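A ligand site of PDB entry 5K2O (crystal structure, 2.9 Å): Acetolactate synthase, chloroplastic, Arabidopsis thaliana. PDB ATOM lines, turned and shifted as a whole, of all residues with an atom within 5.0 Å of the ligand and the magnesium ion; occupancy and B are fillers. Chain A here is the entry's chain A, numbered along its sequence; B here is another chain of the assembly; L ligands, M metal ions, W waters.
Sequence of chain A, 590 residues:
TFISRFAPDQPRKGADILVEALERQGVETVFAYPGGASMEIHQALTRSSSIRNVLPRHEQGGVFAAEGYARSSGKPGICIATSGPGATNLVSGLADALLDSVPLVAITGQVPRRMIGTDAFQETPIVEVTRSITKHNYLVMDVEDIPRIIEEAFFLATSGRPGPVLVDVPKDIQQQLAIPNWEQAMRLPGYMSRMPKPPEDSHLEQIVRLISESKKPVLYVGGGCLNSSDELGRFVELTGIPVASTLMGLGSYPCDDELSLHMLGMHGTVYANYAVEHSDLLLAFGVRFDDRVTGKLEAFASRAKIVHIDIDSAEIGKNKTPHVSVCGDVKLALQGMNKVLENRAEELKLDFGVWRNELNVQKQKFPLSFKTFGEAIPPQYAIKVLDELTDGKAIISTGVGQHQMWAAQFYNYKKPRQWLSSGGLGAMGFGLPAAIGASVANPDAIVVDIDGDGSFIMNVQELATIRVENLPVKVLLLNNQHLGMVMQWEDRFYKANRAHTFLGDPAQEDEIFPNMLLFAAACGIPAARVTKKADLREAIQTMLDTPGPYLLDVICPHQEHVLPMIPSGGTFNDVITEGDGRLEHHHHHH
N of Gly 454 lies close to O2 of the ligand, 2.9 Å away. The backbone NH (N) of His 403 is in hydrogen-bond range of an oxygen (O5) of the ligand, at 2.9 Å. The side-chain carboxylate (OE2) of Glu 59 of chain B is in hydrogen-bond range of a nitrogen (N1) of the ligand. The backbone NH (N) of Gln 402 is in hydrogen-bond range of an oxygen (O6) of the ligand (2.8 Å). O of Val 400 sits close to S1 of the ligand (3.4 Å). An oxygen (O6) of the ligand sits at hydrogen-bond distance from the backbone NH (N) of Gly 484 (3.3 Å). The backbone NH (N) of Met 428 lies within hydrogen-bond range of a nitrogen (N2) of the ligand, 3.2 Å away. O6 of the ligand is in hydrogen-bond range of N of Met 485 (3.1 Å). OG of Ser 455 lies within hydrogen-bond range of O3 of the ligand, 2.6 Å away. The backbone carbonyl oxygen (O) of Gly 426 sits at hydrogen-bond distance from a nitrogen (N3) of the ligand (3.0 Å). The side-chain amide nitrogen (NE2) of Gln 122 of chain B sits close to a nitrogen (N3) of the ligand. The backbone NH of Ser 455 lies within hydrogen-bond range of an oxygen (O3) of the ligand (2.7 Å). ND1 of His 403 sits at hydrogen-bond distance from O4 of the ligand (3.0 Å). O2 of the ligand lies close to N of Asp 453 (3.4 Å).
A ring nitrogen (NE2) of His 403 is in hydrogen-bond range of the backbone NH of Gly 452 (3.1 Å). The side-chain hydroxyl (OG) of Ser 455 is in hydrogen-bond range of the backbone carbonyl oxygen (O) of Val 400 (3.3 Å). The backbone carbonyl oxygen of Gly 426 sits at hydrogen-bond distance from the side-chain amide nitrogen of Gln 122 of chain B, 3.3 Å away. OD2 of Asp 453 sits close to N of Gln 481, 3.3 Å away. OE1 of Glu 59 of chain B sits at hydrogen-bond distance from ND2 of Asn 89 of chain B. The side-chain amide oxygen (OE1) of Gln 402 sits at hydrogen-bond distance from the side-chain amide nitrogen (ND2) of Asn 480. The backbone carbonyl oxygen (O) of Pro 85 of chain B lies close to the side-chain amide nitrogen (ND2) of Asn 89 of chain B (3.4 Å).
Gly 401 touches the ligand. Gly 452 touches the ligand. Met 458 touches the ligand. CA of Leu 483 touches O1 of the ligand, 3.4 Å away. CG2 of Val 486 touches C8 of the ligand, at 3.6 Å. Tyr 33 of chain B touches the ligand. Pro 34 of chain B touches the ligand. Gly 35 of chain B touches the ligand (CA to C6, 3.6 Å). Pro 85 of chain B touches the ligand (CG to N2, 3.6 Å). Asn 89 of chain B touches the ligand (ND2 to C2, 3.4 Å). Of the 32 residues printed, 24 come within 4 Å of the ligand.
Merely in contact with the magnesium ion: Gly 484. Within 4 Å of the magnesium ion: Asp 453, Asn 480, His 482 and Gly 484. The nearest printed residue that does not touch the magnesium ion is Leu 483 (4.2 Å).
O of His 482 binds the magnesium ion (2.0 Å). O7 of the ligand is bound to the magnesium ion (2.0 Å). O2 of the ligand binds the magnesium ion (2.1 Å). The magnesium ion is bound by OD1 of Asn 480 (2.2 Å). OD1 of Asp 453 is bound to the magnesium ion (2.2 Å). Water W1 binds the magnesium ion (2.2 Å).
Water W1 lies within hydrogen-bond range of the backbone carbonyl oxygen (O) of Leu 478 (2.8 Å), an oxygen (O5) of the ligand (3.2 Å) and the backbone NH (N) of Asp 453 (3.3 Å). Water W2 bridges O5 of the ligand and O of Leu 478.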
ATOM      1  N   VAL A 400       2.211   4.259  -6.244  1.00  0.00           N
ATOM      2  CA  VAL A 400       1.225   3.202  -6.418  1.00  0.00           C
ATOM      3  C   VAL A 400       1.673   2.249  -7.508  1.00  0.00           C
ATOM      4  O   VAL A 400       2.115   2.679  -8.579  1.00  0.00           O
ATOM      5  CB  VAL A 400      -0.163   3.775  -6.753  1.00  0.00           C
ATOM      6  CG1 VAL A 400      -1.134   2.678  -7.143  1.00  0.00           C
ATOM      7  CG2 VAL A 400      -0.698   4.572  -5.570  1.00  0.00           C
ATOM      8  N   GLY A 401       1.576   0.955  -7.224  1.00  0.00           N
ATOM      9  CA  GLY A 401       1.988  -0.064  -8.169  1.00  0.00           C
ATOM     10  C   GLY A 401       2.700  -1.215  -7.499  1.00  0.00           C
ATOM     11  O   GLY A 401       2.508  -1.454  -6.305  1.00  0.00           O
ATOM     12  N   GLN A 402       3.523  -1.920  -8.264  1.00  0.00           N
ATOM     13  CA  GLN A 402       4.266  -3.065  -7.745  1.00  0.00           C
ATOM     14  C   GLN A 402       5.188  -2.684  -6.594  1.00  0.00           C
ATOM     15  O   GLN A 402       5.218  -3.373  -5.567  1.00  0.00           O
ATOM     16  CB  GLN A 402       5.085  -3.705  -8.864  1.00  0.00           C
ATOM     17  CG  GLN A 402       4.262  -4.344  -9.959  1.00  0.00           C
ATOM     18  CD  GLN A 402       5.121  -5.077 -10.976  1.00  0.00           C
ATOM     19  OE1 GLN A 402       6.124  -4.538 -11.450  1.00  0.00           O
ATOM     20  NE2 GLN A 402       4.730  -6.299 -11.304  1.00  0.00           N
ATOM     21  N   HIS A 403       5.925  -1.589  -6.755  1.00  0.00           N
ATOM     22  CA  HIS A 403       6.868  -1.136  -5.738  1.00  0.00           C
ATOM     23  C   HIS A 403       6.154  -0.868  -4.419  1.00  0.00           C
ATOM     24  O   HIS A 403       6.708  -1.070  -3.335  1.00  0.00           O
ATOM     25  CB  HIS A 403       7.598   0.137  -6.199  1.00  0.00           C
ATOM     26  CG  HIS A 403       6.713   1.335  -6.298  1.00  0.00           C
ATOM     27  ND1 HIS A 403       5.863   1.561  -7.358  1.00  0.00           N
ATOM     28  CD2 HIS A 403       6.535   2.381  -5.448  1.00  0.00           C
ATOM     29  CE1 HIS A 403       5.206   2.681  -7.165  1.00  0.00           C
ATOM     30  NE2 HIS A 403       5.595   3.204  -6.019  1.00  0.00           N
ATOM     31  N   TRP A 406       5.509  -4.294  -2.743  1.00  0.00           N
ATOM     32  CA  TRP A 406       6.761  -4.828  -2.236  1.00  0.00           C
ATOM     33  C   TRP A 406       7.228  -4.055  -1.012  1.00  0.00           C
ATOM     34  O   TRP A 406       7.821  -4.624  -0.097  1.00  0.00           O
ATOM     35  CB  TRP A 406       7.830  -4.802  -3.329  1.00  0.00           C
ATOM     36  CG  TRP A 406       7.570  -5.802  -4.416  1.00  0.00           C
ATOM     37  CD1 TRP A 406       7.071  -7.057  -4.274  1.00  0.00           C
ATOM     38  CD2 TRP A 406       7.781  -5.618  -5.830  1.00  0.00           C
ATOM     39  NE1 TRP A 406       6.960  -7.677  -5.497  1.00  0.00           N
ATOM     40  CE2 TRP A 406       7.391  -6.812  -6.463  1.00  0.00           C
ATOM     41  CE3 TRP A 406       8.275  -4.565  -6.603  1.00  0.00           C
ATOM     42  CZ2 TRP A 406       7.471  -6.978  -7.849  1.00  0.00           C
ATOM     43  CZ3 TRP A 406       8.348  -4.735  -7.978  1.00  0.00           C
ATOM     44  CH2 TRP A 406       7.951  -5.931  -8.581  1.00  0.00           C
ATOM     45  N   GLY A 426      -5.593   5.103  -4.403  1.00  0.00           N
ATOM     46  CA  GLY A 426      -4.411   4.580  -5.071  1.00  0.00           C
ATOM     47  C   GLY A 426      -3.857   5.534  -6.105  1.00  0.00           C
ATOM     48  O   GLY A 426      -3.713   5.189  -7.276  1.00  0.00           O
ATOM     49  N   ALA A 427      -3.523   6.743  -5.661  1.00  0.00           N
ATOM     50  CA  ALA A 427      -3.069   7.795  -6.569  1.00  0.00           C
ATOM     51  C   ALA A 427      -1.555   7.804  -6.730  1.00  0.00           C
ATOM     52  O   ALA A 427      -0.821   7.971  -5.768  1.00  0.00           O
ATOM     53  CB  ALA A 427      -3.551   9.158  -6.074  1.00  0.00           C
ATOM     54  N   MET A 428      -1.097   7.624  -7.971  1.00  0.00           N
ATOM     55  CA  MET A 428       0.319   7.745  -8.297  1.00  0.00           C
ATOM     56  C   MET A 428       0.812   9.159  -8.024  1.00  0.00           C
ATOM     57  O   MET A 428       0.038  10.107  -7.999  1.00  0.00           O
ATOM     58  CB  MET A 428       0.569   7.388  -9.760  1.00  0.00           C
ATOM     59  CG  MET A 428       0.413   5.916 -10.088  1.00  0.00           C
ATOM     60  SD  MET A 428       0.471   5.635 -11.864  1.00  0.00           S
ATOM     61  CE  MET A 428       2.125   6.213 -12.248  1.00  0.00           C
ATOM     62  N   GLY A 452       8.014   4.220  -7.727  1.00  0.00           N
ATOM     63  CA  GLY A 452       8.145   3.624  -9.049  1.00  0.00           C
ATOM     64  C   GLY A 452       8.466   4.715 -10.045  1.00  0.00           C
ATOM     65  O   GLY A 452       8.214   5.890  -9.771  1.00  0.00           O
ATOM     66  N   ASP A 453       9.027   4.347 -11.196  1.00  0.00           N
ATOM     67  CA  ASP A 453       9.484   5.331 -12.167  1.00  0.00           C
ATOM     68  C   ASP A 453       8.318   6.088 -12.796  1.00  0.00           C
ATOM     69  O   ASP A 453       8.482   7.226 -13.255  1.00  0.00           O
ATOM     70  CB  ASP A 453      10.334   4.673 -13.249  1.00  0.00           C
ATOM     71  CG  ASP A 453       9.633   3.512 -13.922  1.00  0.00           C
ATOM     72  OD1 ASP A 453       8.999   2.704 -13.198  1.00  0.00           O
ATOM     73  OD2 ASP A 453       9.702   3.408 -15.157  1.00  0.00           O
ATOM     74  N   GLY A 454       7.149   5.462 -12.829  1.00  0.00           N
ATOM     75  CA  GLY A 454       5.958   6.124 -13.334  1.00  0.00           C
ATOM     76  C   GLY A 454       5.423   7.100 -12.313  1.00  0.00           C
ATOM     77  O   GLY A 454       5.125   8.255 -12.624  1.00  0.00           O
ATOM     78  N   SER A 455       5.277   6.623 -11.079  1.00  0.00           N
ATOM     79  CA  SER A 455       4.756   7.438  -9.985  1.00  0.00           C
ATOM     80  C   SER A 455       5.674   8.612  -9.666  1.00  0.00           C
ATOM     81  O   SER A 455       5.217   9.723  -9.421  1.00  0.00           O
ATOM     82  CB  SER A 455       4.542   6.575  -8.740  1.00  0.00           C
ATOM     83  OG  SER A 455       3.602   5.547  -8.979  1.00  0.00           O
ATOM     84  N   MET A 458       5.584  11.798 -12.065  1.00  0.00           N
ATOM     85  CA  MET A 458       4.349  12.579 -12.090  1.00  0.00           C
ATOM     86  C   MET A 458       4.451  13.872 -11.301  1.00  0.00           C
ATOM     87  O   MET A 458       3.984  14.924 -11.752  1.00  0.00           O
ATOM     88  CB  MET A 458       3.183  11.759 -11.548  1.00  0.00           C
ATOM     89  CG  MET A 458       2.592  10.772 -12.542  1.00  0.00           C
ATOM     90  SD  MET A 458       0.936  10.256 -12.071  1.00  0.00           S
ATOM     91  CE  MET A 458       0.470   9.282 -13.497  1.00  0.00           C
ATOM     92  N   LEU A 478      12.569   2.366  -7.350  1.00  0.00           N
ATOM     93  CA  LEU A 478      12.617   1.054  -7.983  1.00  0.00           C
ATOM     94  C   LEU A 478      12.220   1.192  -9.439  1.00  0.00           C
ATOM     95  O   LEU A 478      11.033   1.293  -9.765  1.00  0.00           O
ATOM     96  CB  LEU A 478      11.708   0.060  -7.250  1.00  0.00           C
ATOM     97  CG  LEU A 478      12.005  -0.079  -5.750  1.00  0.00           C
ATOM     98  CD1 LEU A 478      11.138  -1.160  -5.124  1.00  0.00           C
ATOM     99  CD2 LEU A 478      13.481  -0.351  -5.510  1.00  0.00           C
ATOM    100  N   ASN A 480      11.709  -0.036 -13.041  1.00  0.00           N
ATOM    101  CA  ASN A 480      11.493  -1.169 -13.935  1.00  0.00           C
ATOM    102  C   ASN A 480      11.133  -0.736 -15.348  1.00  0.00           C
ATOM    103  O   ASN A 480      10.723  -1.553 -16.172  1.00  0.00           O
ATOM    104  CB  ASN A 480      10.406  -2.096 -13.376  1.00  0.00           C
ATOM    105  CG  ASN A 480       9.083  -1.381 -13.141  1.00  0.00           C
ATOM    106  OD1 ASN A 480       8.903  -0.235 -13.541  1.00  0.00           O
ATOM    107  ND2 ASN A 480       8.148  -2.073 -12.501  1.00  0.00           N
ATOM    108  N   GLN A 481      11.280   0.562 -15.619  1.00  0.00           N
ATOM    109  CA  GLN A 481      11.034   1.139 -16.943  1.00  0.00           C
ATOM    110  C   GLN A 481       9.618   0.906 -17.454  1.00  0.00           C
ATOM    111  O   GLN A 481       9.344   1.053 -18.640  1.00  0.00           O
ATOM    112  CB  GLN A 481      12.039   0.593 -17.950  1.00  0.00           C
ATOM    113  CG  GLN A 481      13.470   1.002 -17.669  1.00  0.00           C
ATOM    114  CD  GLN A 481      13.748   2.443 -18.054  1.00  0.00           C
ATOM    115  OE1 GLN A 481      14.118   2.729 -19.189  1.00  0.00           O
ATOM    116  NE2 GLN A 481      13.573   3.350 -17.104  1.00  0.00           N
ATOM    117  N   HIS A 482       8.705   0.540 -16.546  1.00  0.00           N
ATOM    118  CA  HIS A 482       7.344   0.202 -16.924  1.00  0.00           C
ATOM    119  C   HIS A 482       6.320   0.734 -15.917  1.00  0.00           C
ATOM    120  O   HIS A 482       6.654   1.040 -14.782  1.00  0.00           O
ATOM    121  CB  HIS A 482       7.176  -1.310 -17.052  1.00  0.00           C
ATOM    122  CG  HIS A 482       7.768  -1.890 -18.299  1.00  0.00           C
ATOM    123  ND1 HIS A 482       9.124  -2.024 -18.481  1.00  0.00           N
ATOM    124  CD2 HIS A 482       7.182  -2.383 -19.413  1.00  0.00           C
ATOM    125  CE1 HIS A 482       9.347  -2.578 -19.660  1.00  0.00           C
ATOM    126  NE2 HIS A 482       8.194  -2.796 -20.252  1.00  0.00           N
ATOM    127  N   LEU A 483       5.073   0.819 -16.359  1.00  0.00           N
ATOM    128  CA  LEU A 483       3.955   0.907 -15.436  1.00  0.00           C
ATOM    129  C   LEU A 483       3.700  -0.512 -14.936  1.00  0.00           C
ATOM    130  O   LEU A 483       2.828  -1.220 -15.429  1.00  0.00           O
ATOM    131  CB  LEU A 483       2.720   1.498 -16.110  1.00  0.00           C
ATOM    132  CG  LEU A 483       2.876   2.946 -16.562  1.00  0.00           C
ATOM    133  CD1 LEU A 483       1.668   3.408 -17.357  1.00  0.00           C
ATOM    134  CD2 LEU A 483       3.103   3.860 -15.370  1.00  0.00           C
ATOM    135  N   GLY A 484       4.490  -0.909 -13.944  1.00  0.00           N
ATOM    136  CA  GLY A 484       4.647  -2.299 -13.546  1.00  0.00           C
ATOM    137  C   GLY A 484       3.400  -3.120 -13.256  1.00  0.00           C
ATOM    138  O   GLY A 484       3.277  -4.244 -13.754  1.00  0.00           O
ATOM    139  N   MET A 485       2.498  -2.572 -12.461  1.00  0.00           N
ATOM    140  CA  MET A 485       1.302  -3.313 -12.055  1.00  0.00           C
ATOM    141  C   MET A 485       0.344  -3.534 -13.216  1.00  0.00           C
ATOM    142  O   MET A 485      -0.287  -4.587 -13.328  1.00  0.00           O
ATOM    143  CB  MET A 485       0.584  -2.582 -10.907  1.00  0.00           C
ATOM    144  CG  MET A 485      -0.643  -3.316 -10.380  1.00  0.00           C
ATOM    145  SD  MET A 485      -0.297  -4.962  -9.739  1.00  0.00           S
ATOM    146  CE  MET A 485       0.793  -4.579  -8.363  1.00  0.00           C
ATOM    147  N   VAL A 486       0.242  -2.543 -14.098  1.00  0.00           N
ATOM    148  CA  VAL A 486      -0.587  -2.666 -15.287  1.00  0.00           C
ATOM    149  C   VAL A 486       0.054  -3.693 -16.213  1.00  0.00           C
ATOM    150  O   VAL A 486      -0.626  -4.485 -16.862  1.00  0.00           O
ATOM    151  CB  VAL A 486      -0.762  -1.320 -16.024  1.00  0.00           C
ATOM    152  CG1 VAL A 486      -1.686  -1.473 -17.219  1.00  0.00           C
ATOM    153  CG2 VAL A 486      -1.293  -0.267 -15.068  1.00  0.00           C
ATOM    154  N   LEU A 503       7.709   2.788 -20.283  1.00  0.00           N
ATOM    155  CA  LEU A 503       7.960   4.196 -19.981  1.00  0.00           C
ATOM    156  C   LEU A 503       9.290   4.703 -20.524  1.00  0.00           C
ATOM    157  O   LEU A 503       9.609   5.887 -20.368  1.00  0.00           O
ATOM    158  CB  LEU A 503       7.898   4.426 -18.478  1.00  0.00           C
ATOM    159  CG  LEU A 503       6.537   4.287 -17.813  1.00  0.00           C
ATOM    160  CD1 LEU A 503       6.672   4.382 -16.310  1.00  0.00           C
ATOM    161  CD2 LEU A 503       5.577   5.344 -18.325  1.00  0.00           C
ATOM    162  N   TYR B  33      -3.789   7.468 -20.751  1.00  0.00           N
ATOM    163  CA  TYR B  33      -2.897   6.947 -19.716  1.00  0.00           C
ATOM    164  C   TYR B  33      -3.564   5.759 -19.028  1.00  0.00           C
ATOM    165  O   TYR B  33      -4.616   5.911 -18.392  1.00  0.00           O
ATOM    166  CB  TYR B  33      -2.549   8.042 -18.716  1.00  0.00           C
ATOM    167  CG  TYR B  33      -1.345   7.754 -17.856  1.00  0.00           C
ATOM    168  CD1 TYR B  33      -1.445   6.959 -16.719  1.00  0.00           C
ATOM    169  CD2 TYR B  33      -0.091   8.272 -18.176  1.00  0.00           C
ATOM    170  CE1 TYR B  33      -0.348   6.687 -15.933  1.00  0.00           C
ATOM    171  CE2 TYR B  33       1.011   8.013 -17.391  1.00  0.00           C
ATOM    172  CZ  TYR B  33       0.883   7.220 -16.278  1.00  0.00           C
ATOM    173  OH  TYR B  33       1.985   6.961 -15.493  1.00  0.00           O
ATOM    174  N   PRO B  34      -2.964   4.575 -19.147  1.00  0.00           N
ATOM    175  CA  PRO B  34      -3.618   3.321 -18.737  1.00  0.00           C
ATOM    176  C   PRO B  34      -3.768   3.158 -17.230  1.00  0.00           C
ATOM    177  O   PRO B  34      -2.991   3.699 -16.440  1.00  0.00           O
ATOM    178  CB  PRO B  34      -2.682   2.241 -19.291  1.00  0.00           C
ATOM    179  CG  PRO B  34      -1.352   2.901 -19.349  1.00  0.00           C
ATOM    180  CD  PRO B  34      -1.615   4.330 -19.702  1.00  0.00           C
ATOM    181  N   GLY B  35      -4.780   2.385 -16.857  1.00  0.00           N
ATOM    182  CA  GLY B  35      -5.005   1.997 -15.476  1.00  0.00           C
ATOM    183  C   GLY B  35      -5.908   0.787 -15.501  1.00  0.00           C
ATOM    184  O   GLY B  35      -6.490   0.460 -16.531  1.00  0.00           O
ATOM    185  N   GLY B  36      -6.031   0.109 -14.363  1.00  0.00           N
ATOM    186  CA  GLY B  36      -6.805  -1.123 -14.278  1.00  0.00           C
ATOM    187  C   GLY B  36      -8.227  -1.002 -14.792  1.00  0.00           C
ATOM    188  O   GLY B  36      -8.754  -1.931 -15.406  1.00  0.00           O
ATOM    189  N   GLU B  59      -1.958  12.604 -16.338  1.00  0.00           N
ATOM    190  CA  GLU B  59      -3.239  12.798 -17.018  1.00  0.00           C
ATOM    191  C   GLU B  59      -3.582  14.272 -17.214  1.00  0.00           C
ATOM    192  O   GLU B  59      -4.336  14.608 -18.130  1.00  0.00           O
ATOM    193  CB  GLU B  59      -4.362  12.109 -16.255  1.00  0.00           C
ATOM    194  CG  GLU B  59      -4.330  10.595 -16.336  1.00  0.00           C
ATOM    195  CD  GLU B  59      -3.610   9.957 -15.168  1.00  0.00           C
ATOM    196  OE1 GLU B  59      -2.890  10.662 -14.441  1.00  0.00           O
ATOM    197  OE2 GLU B  59      -3.779   8.730 -14.979  1.00  0.00           O
ATOM    198  N   THR B  82      -7.917   6.397 -16.510  1.00  0.00           N
ATOM    199  CA  THR B  82      -8.532   5.341 -15.723  1.00  0.00           C
ATOM    200  C   THR B  82      -9.438   5.937 -14.642  1.00  0.00           C
ATOM    201  O   THR B  82      -9.558   7.160 -14.531  1.00  0.00           O
ATOM    202  CB  THR B  82      -7.475   4.437 -15.077  1.00  0.00           C
ATOM    203  OG1 THR B  82      -8.075   3.207 -14.663  1.00  0.00           O
ATOM    204  CG2 THR B  82      -6.816   5.120 -13.892  1.00  0.00           C
ATOM    205  N   PRO B  85      -8.034   8.230  -9.431  1.00  0.00           N
ATOM    206  CA  PRO B  85      -6.922   9.185  -9.517  1.00  0.00           C
ATOM    207  C   PRO B  85      -6.613   9.587 -10.954  1.00  0.00           C
ATOM    208  O   PRO B  85      -6.073  10.666 -11.183  1.00  0.00           O
ATOM    209  CB  PRO B  85      -5.760   8.406  -8.897  1.00  0.00           C
ATOM    210  CG  PRO B  85      -6.109   6.977  -9.101  1.00  0.00           C
ATOM    211  CD  PRO B  85      -7.602   6.912  -8.945  1.00  0.00           C
ATOM    212  N   GLY B  86      -6.942   8.711 -11.904  1.00  0.00           N
ATOM    213  CA  GLY B  86      -6.818   9.054 -13.306  1.00  0.00           C
ATOM    214  C   GLY B  86      -7.819  10.133 -13.665  1.00  0.00           C
ATOM    215  O   GLY B  86      -7.458  11.157 -14.253  1.00  0.00           O
ATOM    216  N   ASN B  89      -7.329  13.606 -12.101  1.00  0.00           N
ATOM    217  CA  ASN B  89      -6.188  14.294 -12.684  1.00  0.00           C
ATOM    218  C   ASN B  89      -6.549  15.037 -13.968  1.00  0.00           C
ATOM    219  O   ASN B  89      -5.730  15.784 -14.512  1.00  0.00           O
ATOM    220  CB  ASN B  89      -5.055  13.309 -12.957  1.00  0.00           C
ATOM    221  CG  ASN B  89      -4.104  13.166 -11.786  1.00  0.00           C
ATOM    222  OD1 ASN B  89      -4.236  13.860 -10.780  1.00  0.00           O
ATOM    223  ND2 ASN B  89      -3.129  12.273 -11.915  1.00  0.00           N
ATOM    224  N   GLN B 122     -10.227   2.729  -6.292  1.00  0.00           N
ATOM    225  CA  GLN B 122     -10.083   3.761  -7.316  1.00  0.00           C
ATOM    226  C   GLN B 122     -11.424   4.228  -7.872  1.00  0.00           C
ATOM    227  O   GLN B 122     -11.581   4.410  -9.081  1.00  0.00           O
ATOM    228  CB  GLN B 122      -9.195   3.244  -8.456  1.00  0.00           C
ATOM    229  CG  GLN B 122      -7.825   2.787  -8.000  1.00  0.00           C
ATOM    230  CD  GLN B 122      -6.854   2.603  -9.151  1.00  0.00           C
ATOM    231  OE1 GLN B 122      -7.182   1.983 -10.159  1.00  0.00           O
ATOM    232  NE2 GLN B 122      -5.654   3.150  -8.999  1.00  0.00           N
HETATM  233  N1  LIG L   1      -2.857   7.440 -12.690  1.00  0.00           N
HETATM  234  C1  LIG L   1      -2.780   7.620 -11.387  1.00  0.00           C
HETATM  235  C2  LIG L   1      -2.655   9.036 -10.858  1.00  0.00           C
HETATM  236  N2  LIG L   1      -2.818   6.616 -10.531  1.00  0.00           N
HETATM  237  C3  LIG L   1      -2.930   5.348 -10.952  1.00  0.00           C
HETATM  238  N3  LIG L   1      -2.969   4.289 -10.021  1.00  0.00           N
HETATM  239  C4  LIG L   1      -3.018   5.104 -12.341  1.00  0.00           C
HETATM  240  C5  LIG L   1      -2.971   6.203 -13.212  1.00  0.00           C
HETATM  241  C6  LIG L   1      -3.145   3.707 -12.925  1.00  0.00           C
HETATM  242  N4  LIG L   1      -2.220   2.791 -12.351  1.00  0.00           N
HETATM  243  S1  LIG L   1      -0.164   1.158 -10.637  1.00  0.00           S
HETATM  244  C7  LIG L   1       0.060   1.929 -12.203  1.00  0.00           C
HETATM  245  C8  LIG L   1      -0.902   2.608 -12.861  1.00  0.00           C
HETATM  246  C9  LIG L   1      -0.726   3.286 -14.205  1.00  0.00           C
HETATM  247  C10 LIG L   1       1.488   1.718 -12.684  1.00  0.00           C
HETATM  248  C11 LIG L   1       2.476   2.605 -11.955  1.00  0.00           C
HETATM  249  O1  LIG L   1       3.778   2.204 -12.300  1.00  0.00           O
HETATM  250  P1  LIG L   1       4.987   2.657 -11.368  1.00  0.00           P
HETATM  251  O2  LIG L   1       6.239   2.781 -12.203  1.00  0.00           O
HETATM  252  O3  LIG L   1       4.667   3.974 -10.720  1.00  0.00           O
HETATM  253  O4  LIG L   1       5.215   1.557 -10.246  1.00  0.00           O
HETATM  254  P2  LIG L   1       5.465   0.033 -10.570  1.00  0.00           P
HETATM  255  O5  LIG L   1       6.274  -0.569  -9.448  1.00  0.00           O
HETATM  256  O6  LIG L   1       4.154  -0.695 -10.684  1.00  0.00           O
HETATM  257  O7  LIG L   1       6.229  -0.084 -11.860  1.00  0.00           O
HETATM  258 MG    MG M   1       7.400   1.221 -12.916  1.00  0.00          MG
HETATM  259  O   HOH W   1       8.558   1.106 -11.005  1.00  0.00           O
HETATM  260  O   HOH W   2       8.781  -1.186  -9.096  1.00  0.00           O
